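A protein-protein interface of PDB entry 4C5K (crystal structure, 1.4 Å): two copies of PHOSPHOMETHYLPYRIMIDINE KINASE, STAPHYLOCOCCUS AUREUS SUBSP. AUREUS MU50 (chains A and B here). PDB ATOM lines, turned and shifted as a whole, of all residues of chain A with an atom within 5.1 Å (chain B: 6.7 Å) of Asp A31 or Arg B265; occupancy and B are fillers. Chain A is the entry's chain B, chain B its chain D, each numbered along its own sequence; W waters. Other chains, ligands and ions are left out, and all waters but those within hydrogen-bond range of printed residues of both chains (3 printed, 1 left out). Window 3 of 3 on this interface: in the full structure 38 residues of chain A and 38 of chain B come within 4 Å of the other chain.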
ATOM      1  N   LEU A   3       1.016  -1.853 -16.015  1.00  0.00           N
ATOM      2  CA  LEU A   3       0.443  -1.991 -17.374  1.00  0.00           C
ATOM      3  C   LEU A   3       1.463  -2.551 -18.323  1.00  0.00           C
ATOM      4  O   LEU A   3       2.617  -2.174 -18.333  1.00  0.00           O
ATOM      5  CB  LEU A   3      -0.002  -0.634 -17.913  1.00  0.00           C
ATOM      6  CG  LEU A   3      -1.131   0.088 -17.182  1.00  0.00           C
ATOM      7  CD1 LEU A   3      -1.303   1.497 -17.714  1.00  0.00           C
ATOM      8  CD2 LEU A   3      -2.448  -0.674 -17.335  1.00  0.00           C
ATOM      9  N   LYS A   4       1.005  -3.491 -19.127  1.00  0.00           N
ATOM     10  CA  LYS A   4       1.855  -3.986 -20.177  1.00  0.00           C
ATOM     11  C   LYS A   4       1.976  -2.939 -21.293  1.00  0.00           C
ATOM     12  O   LYS A   4       0.991  -2.331 -21.674  1.00  0.00           O
ATOM     13  CB  LYS A   4       1.261  -5.250 -20.726  1.00  0.00           C
ATOM     14  CG  LYS A   4       1.219  -6.360 -19.714  1.00  0.00           C
ATOM     15  CD  LYS A   4       2.548  -6.843 -19.298  1.00  0.00           C
ATOM     16  CE  LYS A   4       2.382  -8.019 -18.346  1.00  0.00           C
ATOM     17  NZ  LYS A   4       3.746  -8.470 -18.043  1.00  0.00           N
ATOM     18  N   PHE A  27      -5.997  -1.173 -27.560  1.00  0.00           N
ATOM     19  CA  PHE A  27      -5.056  -1.331 -26.461  1.00  0.00           C
ATOM     20  C   PHE A  27      -5.593  -0.730 -25.146  1.00  0.00           C
ATOM     21  O   PHE A  27      -5.435  -1.284 -24.080  1.00  0.00           O
ATOM     22  CB  PHE A  27      -3.703  -0.714 -26.788  1.00  0.00           C
ATOM     23  CG  PHE A  27      -2.985  -1.334 -27.966  1.00  0.00           C
ATOM     24  CD1 PHE A  27      -3.239  -2.622 -28.437  1.00  0.00           C
ATOM     25  CD2 PHE A  27      -2.006  -0.612 -28.604  1.00  0.00           C
ATOM     26  CE1 PHE A  27      -2.557  -3.130 -29.519  1.00  0.00           C
ATOM     27  CE2 PHE A  27      -1.279  -1.111 -29.679  1.00  0.00           C
ATOM     28  CZ  PHE A  27      -1.566  -2.392 -30.138  1.00  0.00           C
ATOM     29  N   GLN A  28      -6.191   0.439 -25.265  1.00  0.00           N
ATOM     30  CA  GLN A  28      -6.764   1.165 -24.111  1.00  0.00           C
ATOM     31  C   GLN A  28      -7.927   0.413 -23.514  1.00  0.00           C
ATOM     32  O   GLN A  28      -8.035   0.211 -22.311  1.00  0.00           O
ATOM     33  CB  GLN A  28      -7.202   2.574 -24.519  1.00  0.00           C
ATOM     34  CG  GLN A  28      -7.517   3.479 -23.339  1.00  0.00           C
ATOM     35  CD  GLN A  28      -6.282   3.735 -22.477  1.00  0.00           C
ATOM     36  OE1 GLN A  28      -5.141   3.715 -22.943  1.00  0.00           O
ATOM     37  NE2 GLN A  28      -6.525   3.937 -21.221  1.00  0.00           N
ATOM     38  N   GLU A  29      -8.827  -0.048 -24.374  1.00  0.00           N
ATOM     39  CA  GLU A  29      -9.981  -0.873 -23.961  1.00  0.00           C
ATOM     40  C   GLU A  29      -9.533  -2.118 -23.199  1.00  0.00           C
ATOM     41  O   GLU A  29     -10.232  -2.620 -22.307  1.00  0.00           O
ATOM     42  CB  GLU A  29     -10.809  -1.268 -25.190  1.00  0.00           C
ATOM     43  CG  GLU A  29     -11.621  -0.134 -25.785  1.00  0.00           C
ATOM     44  CD  GLU A  29     -12.771   0.329 -24.920  1.00  0.00           C
ATOM     45  OE1 GLU A  29     -13.277  -0.489 -24.110  1.00  0.00           O
ATOM     46  OE2 GLU A  29     -13.226   1.491 -25.088  1.00  0.00           O
ATOM     47  N   LEU A  30      -8.406  -2.673 -23.595  1.00  0.00           N
ATOM     48  CA  LEU A  30      -7.909  -3.879 -22.986  1.00  0.00           C
ATOM     49  C   LEU A  30      -6.849  -3.686 -21.924  1.00  0.00           C
ATOM     50  O   LEU A  30      -6.070  -4.596 -21.575  1.00  0.00           O
ATOM     51  CB  LEU A  30      -7.452  -4.876 -24.079  1.00  0.00           C
ATOM     52  CG  LEU A  30      -8.608  -5.306 -24.972  1.00  0.00           C
ATOM     53  CD1 LEU A  30      -8.120  -6.100 -26.178  1.00  0.00           C
ATOM     54  CD2 LEU A  30      -9.618  -6.116 -24.179  1.00  0.00           C
ATOM     55  N   ASP A  31      -6.827  -2.464 -21.377  1.00  0.00           N
ATOM     56  CA  ASP A  31      -6.104  -2.235 -20.150  1.00  0.00           C
ATOM     57  C   ASP A  31      -4.621  -2.459 -20.297  1.00  0.00           C
ATOM     58  O   ASP A  31      -3.976  -3.028 -19.419  1.00  0.00           O
ATOM     59  CB  ASP A  31      -6.706  -3.023 -18.983  1.00  0.00           C
ATOM     60  CG  ASP A  31      -8.117  -2.630 -18.672  1.00  0.00           C
ATOM     61  OD1 ASP A  31      -8.464  -1.432 -18.830  1.00  0.00           O
ATOM     62  OD2 ASP A  31      -8.844  -3.544 -18.247  1.00  0.00           O
ATOM     63  N   THR A  32      -4.077  -1.977 -21.446  1.00  0.00           N
ATOM     64  CA  THR A  32      -2.653  -1.979 -21.688  1.00  0.00           C
ATOM     65  C   THR A  32      -2.207  -0.520 -21.949  1.00  0.00           C
ATOM     66  O   THR A  32      -3.037   0.353 -22.110  1.00  0.00           O
ATOM     67  CB  THR A  32      -2.255  -2.843 -22.903  1.00  0.00           C
ATOM     68  OG1 THR A  32      -2.805  -2.311 -24.108  1.00  0.00           O
ATOM     69  CG2 THR A  32      -2.675  -4.322 -22.692  1.00  0.00           C
ATOM     70  N   TYR A  33      -0.892  -0.309 -21.985  1.00  0.00           N
ATOM     71  CA  TYR A  33      -0.300   1.000 -22.238  1.00  0.00           C
ATOM     72  C   TYR A  33       0.064   1.053 -23.736  1.00  0.00           C
ATOM     73  O   TYR A  33       1.071   0.479 -24.157  1.00  0.00           O
ATOM     74  CB  TYR A  33       0.917   1.270 -21.403  1.00  0.00           C
ATOM     75  CG  TYR A  33       1.468   2.665 -21.608  1.00  0.00           C
ATOM     76  CD1 TYR A  33       0.874   3.770 -20.990  1.00  0.00           C
ATOM     77  CD2 TYR A  33       2.555   2.896 -22.404  1.00  0.00           C
ATOM     78  CE1 TYR A  33       1.374   5.036 -21.181  1.00  0.00           C
ATOM     79  CE2 TYR A  33       3.074   4.195 -22.598  1.00  0.00           C
ATOM     80  CZ  TYR A  33       2.459   5.242 -21.971  1.00  0.00           C
ATOM     81  OH  TYR A  33       2.893   6.533 -22.090  1.00  0.00           O
ATOM     82  N   ASN A 226      -1.342  -9.501 -21.859  1.00  0.00           N
ATOM     83  CA  ASN A 226      -1.979  -9.665 -20.550  1.00  0.00           C
ATOM     84  C   ASN A 226      -2.087 -11.106 -20.078  1.00  0.00           C
ATOM     85  O   ASN A 226      -2.666 -11.366 -19.014  1.00  0.00           O
ATOM     86  CB  ASN A 226      -3.341  -8.994 -20.541  1.00  0.00           C
ATOM     87  CG  ASN A 226      -3.255  -7.509 -20.452  1.00  0.00           C
ATOM     88  OD1 ASN A 226      -2.290  -6.979 -19.970  1.00  0.00           O
ATOM     89  ND2 ASN A 226      -4.276  -6.845 -20.912  1.00  0.00           N
ATOM     90  N   GLU B  29     -11.736   6.298 -23.144  1.00  0.00           N
ATOM     91  CA  GLU B  29     -12.182   6.013 -21.793  1.00  0.00           C
ATOM     92  C   GLU B  29     -13.511   6.653 -21.475  1.00  0.00           C
ATOM     93  O   GLU B  29     -14.253   6.114 -20.633  1.00  0.00           O
ATOM     94  CB  GLU B  29     -11.157   6.528 -20.789  1.00  0.00           C
ATOM     95  CG  GLU B  29      -9.884   5.729 -20.660  1.00  0.00           C
ATOM     96  CD  GLU B  29     -10.093   4.327 -20.077  1.00  0.00           C
ATOM     97  OE1 GLU B  29     -10.994   4.183 -19.228  1.00  0.00           O
ATOM     98  OE2 GLU B  29      -9.246   3.464 -20.391  1.00  0.00           O
ATOM     99  N   ASN B 247      -2.356   7.283  -9.924  1.00  0.00           N
ATOM    100  CA  ASN B 247      -1.924   6.020 -10.457  1.00  0.00           C
ATOM    101  C   ASN B 247      -0.858   6.103 -11.532  1.00  0.00           C
ATOM    102  O   ASN B 247      -0.599   5.139 -12.260  1.00  0.00           O
ATOM    103  CB  ASN B 247      -3.135   5.213 -10.913  1.00  0.00           C
ATOM    104  CG  ASN B 247      -4.000   4.826  -9.735  1.00  0.00           C
ATOM    105  OD1 ASN B 247      -3.581   3.921  -8.983  1.00  0.00           O
ATOM    106  ND2 ASN B 247      -5.091   5.539  -9.486  1.00  0.00           N
ATOM    107  N   ASP B 259      -1.928   7.406 -15.576  1.00  0.00           N
ATOM    108  CA  ASP B 259      -2.656   6.245 -16.050  1.00  0.00           C
ATOM    109  C   ASP B 259      -4.030   6.678 -16.474  1.00  0.00           C
ATOM    110  O   ASP B 259      -4.977   6.832 -15.703  1.00  0.00           O
ATOM    111  CB  ASP B 259      -2.733   5.193 -14.932  1.00  0.00           C
ATOM    112  CG  ASP B 259      -3.428   3.920 -15.350  1.00  0.00           C
ATOM    113  OD1 ASP B 259      -4.125   3.916 -16.373  1.00  0.00           O
ATOM    114  OD2 ASP B 259      -3.331   2.932 -14.600  1.00  0.00           O
ATOM    115  N   HIS B 260      -4.193   6.912 -17.797  1.00  0.00           N
ATOM    116  CA  HIS B 260      -5.387   7.512 -18.331  1.00  0.00           C
ATOM    117  C   HIS B 260      -6.667   6.740 -18.012  1.00  0.00           C
ATOM    118  O   HIS B 260      -7.743   7.314 -17.931  1.00  0.00           O
ATOM    119  CB  HIS B 260      -5.279   7.728 -19.868  1.00  0.00           C
ATOM    120  CG  HIS B 260      -3.986   8.262 -20.310  1.00  0.00           C
ATOM    121  ND1 HIS B 260      -2.865   7.474 -20.434  1.00  0.00           N
ATOM    122  CD2 HIS B 260      -3.593   9.548 -20.511  1.00  0.00           C
ATOM    123  CE1 HIS B 260      -1.853   8.239 -20.782  1.00  0.00           C
ATOM    124  NE2 HIS B 260      -2.257   9.503 -20.791  1.00  0.00           N
ATOM    125  N   GLY B 261      -6.515   5.419 -17.866  1.00  0.00           N
ATOM    126  CA  GLY B 261      -7.614   4.565 -17.573  1.00  0.00           C
ATOM    127  C   GLY B 261      -7.926   4.345 -16.078  1.00  0.00           C
ATOM    128  O   GLY B 261      -8.830   3.579 -15.767  1.00  0.00           O
ATOM    129  N   ALA B 262      -7.225   5.050 -15.199  1.00  0.00           N
ATOM    130  CA  ALA B 262      -7.382   4.783 -13.756  1.00  0.00           C
ATOM    131  C   ALA B 262      -8.729   5.110 -13.222  1.00  0.00           C
ATOM    132  O   ALA B 262      -9.241   4.410 -12.350  1.00  0.00           O
ATOM    133  CB  ALA B 262      -6.320   5.491 -12.972  1.00  0.00           C
ATOM    134  N   TYR B 263      -9.390   6.192 -13.684  1.00  0.00           N
ATOM    135  CA  TYR B 263     -10.685   6.554 -13.218  1.00  0.00           C
ATOM    136  C   TYR B 263     -11.680   5.393 -13.338  1.00  0.00           C
ATOM    137  O   TYR B 263     -12.449   5.120 -12.439  1.00  0.00           O
ATOM    138  CB  TYR B 263     -11.209   7.796 -13.916  1.00  0.00           C
ATOM    139  CG  TYR B 263     -12.527   8.287 -13.377  1.00  0.00           C
ATOM    140  CD1 TYR B 263     -12.589   9.118 -12.283  1.00  0.00           C
ATOM    141  CD2 TYR B 263     -13.720   7.983 -14.007  1.00  0.00           C
ATOM    142  CE1 TYR B 263     -13.780   9.567 -11.776  1.00  0.00           C
ATOM    143  CE2 TYR B 263     -14.924   8.424 -13.507  1.00  0.00           C
ATOM    144  CZ  TYR B 263     -14.961   9.235 -12.376  1.00  0.00           C
ATOM    145  OH  TYR B 263     -16.193   9.643 -11.885  1.00  0.00           O
ATOM    146  N   ASN B 264     -11.643   4.685 -14.474  1.00  0.00           N
ATOM    147  CA  ASN B 264     -12.582   3.610 -14.748  1.00  0.00           C
ATOM    148  C   ASN B 264     -12.099   2.270 -14.215  1.00  0.00           C
ATOM    149  O   ASN B 264     -12.926   1.462 -13.792  1.00  0.00           O
ATOM    150  CB  ASN B 264     -12.878   3.515 -16.246  1.00  0.00           C
ATOM    151  CG  ASN B 264     -13.687   4.704 -16.766  1.00  0.00           C
ATOM    152  OD1 ASN B 264     -14.548   5.255 -16.062  1.00  0.00           O
ATOM    153  ND2 ASN B 264     -13.434   5.096 -18.013  1.00  0.00           N
ATOM    154  N   ARG B 265     -10.812   2.040 -14.244  1.00  0.00           N
ATOM    155  CA  ARG B 265     -10.226   0.739 -13.906  1.00  0.00           C
ATOM    156  C   ARG B 265      -9.887   0.590 -12.439  1.00  0.00           C
ATOM    157  O   ARG B 265      -9.922  -0.541 -11.893  1.00  0.00           O
ATOM    158  CB  ARG B 265      -8.963   0.482 -14.727  1.00  0.00           C
ATOM    159  CG  ARG B 265      -8.622  -0.983 -14.891  1.00  0.00           C
ATOM    160  CD  ARG B 265      -7.380  -1.144 -15.756  1.00  0.00           C
ATOM    161  NE  ARG B 265      -6.138  -0.773 -15.074  1.00  0.00           N
ATOM    162  CZ  ARG B 265      -5.457   0.362 -15.226  1.00  0.00           C
ATOM    163  NH1 ARG B 265      -5.860   1.332 -16.070  1.00  0.00           N
ATOM    164  NH2 ARG B 265      -4.345   0.518 -14.507  1.00  0.00           N
ATOM    165  N   ILE B 266      -9.528   1.698 -11.777  1.00  0.00           N
ATOM    166  CA  ILE B 266      -8.974   1.639 -10.437  1.00  0.00           C
ATOM    167  C   ILE B 266      -9.847   2.323  -9.420  1.00  0.00           C
ATOM    168  O   ILE B 266     -10.259   1.702  -8.447  1.00  0.00           O
ATOM    169  CB  ILE B 266      -7.544   2.198 -10.356  1.00  0.00           C
ATOM    170  CG1 ILE B 266      -6.603   1.458 -11.307  1.00  0.00           C
ATOM    171  CG2 ILE B 266      -7.011   2.096  -8.957  1.00  0.00           C
ATOM    172  CD1 ILE B 266      -5.189   1.960 -11.388  1.00  0.00           C
ATOM    173  N   GLU B 267     -10.118   3.620  -9.590  1.00  0.00           N
ATOM    174  CA  GLU B 267     -10.818   4.382  -8.572  1.00  0.00           C
ATOM    175  C   GLU B 267     -11.278   5.740  -9.036  1.00  0.00           C
ATOM    176  O   GLU B 267     -10.588   6.408  -9.859  1.00  0.00           O
ATOM    177  CB  GLU B 267      -9.919   4.521  -7.339  1.00  0.00           C
ATOM    178  CG  GLU B 267      -8.750   5.492  -7.551  1.00  0.00           C
ATOM    179  CD  GLU B 267      -7.653   5.361  -6.532  1.00  0.00           C
ATOM    180  OE1 GLU B 267      -7.983   5.450  -5.320  1.00  0.00           O
ATOM    181  OE2 GLU B 267      -6.492   5.115  -6.896  1.00  0.00           O
HETATM  182  O   HOH W   1     -10.508   0.880 -20.884  1.00  0.00           O
HETATM  183  O   HOH W   2     -11.022   2.482 -22.825  1.00  0.00           O
HETATM  184  O   HOH W   3      -4.344   3.493 -19.067  1.00  0.00           O
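NE2 of Gln A28 sits at hydrogen-bond distance from OE2 of Glu B29, 2.9 Å away.
Water W3 lies within hydrogen-bond range of OD1 of Asp B259, NE2 of Gln A28 and N of Gly B261.
Water W1 lies within hydrogen-bond range of the side-chain carboxylate (OE2) of Glu B29 (2.9 Å) and the backbone carbonyl oxygen (O) of Gln A28 (2.9 Å).
Water W2 lies within hydrogen-bond range of OE2 of Glu B29 and OE2 of Glu A29.
Of the 10 printed residues of chain A, 3 touch a printed residue of chain B.
Among the printed residues, 5 pairs touch across the chains.
Among the printed residues, no Asp or Glu carboxylate lies within 4 Å of a Lys or Arg side-chain nitrogen of the other chain.
1 position is printed for both chains.
Leu A3 touches Asp B259.
CD2 of Leu A3 touches NH2 of Arg B265 (3.6 Å).
Gly B261 touches Gln A28.
OD1 of Asp A31 touches CD of Arg B265 (3.3 Å).
Printed residues of chain B within 4 Å of Leu A3: Asp B259 (3.95 Å) and Arg B265 (3.6 Å).
Of the printed residues of chain B, Gln A28 touches Glu B29 (2.9 Å) and Gly B261 (3.7 Å).
Of the printed residues of chain B, Asp A31 touches Arg B265.
Thr A32 touches none of the printed residues of chain B.
Of the printed residues of chain A, Asp B259 touches Leu A3 (3.95 Å).
Printed residues of chain A within 4 Å of Gly B261: Gln A28 (3.7 Å).
Tyr B263 touches none of the printed residues of chain A.
Of the printed residues of chain A, Arg B265 touches Leu A3 and Asp A31.
The side-chain carboxylate (OE1) of Glu B29 lies within hydrogen-bond range of the side-chain amide nitrogen (ND2) of Asn B264 (2.9 Å).
NH2 of Arg B265 is in salt-bridge range of OD2 of Asp B259, 2.6 Å away.
The side-chain carboxylate of Asp B259 sits close to the backbone NH of Gly B261 (3.2 Å).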
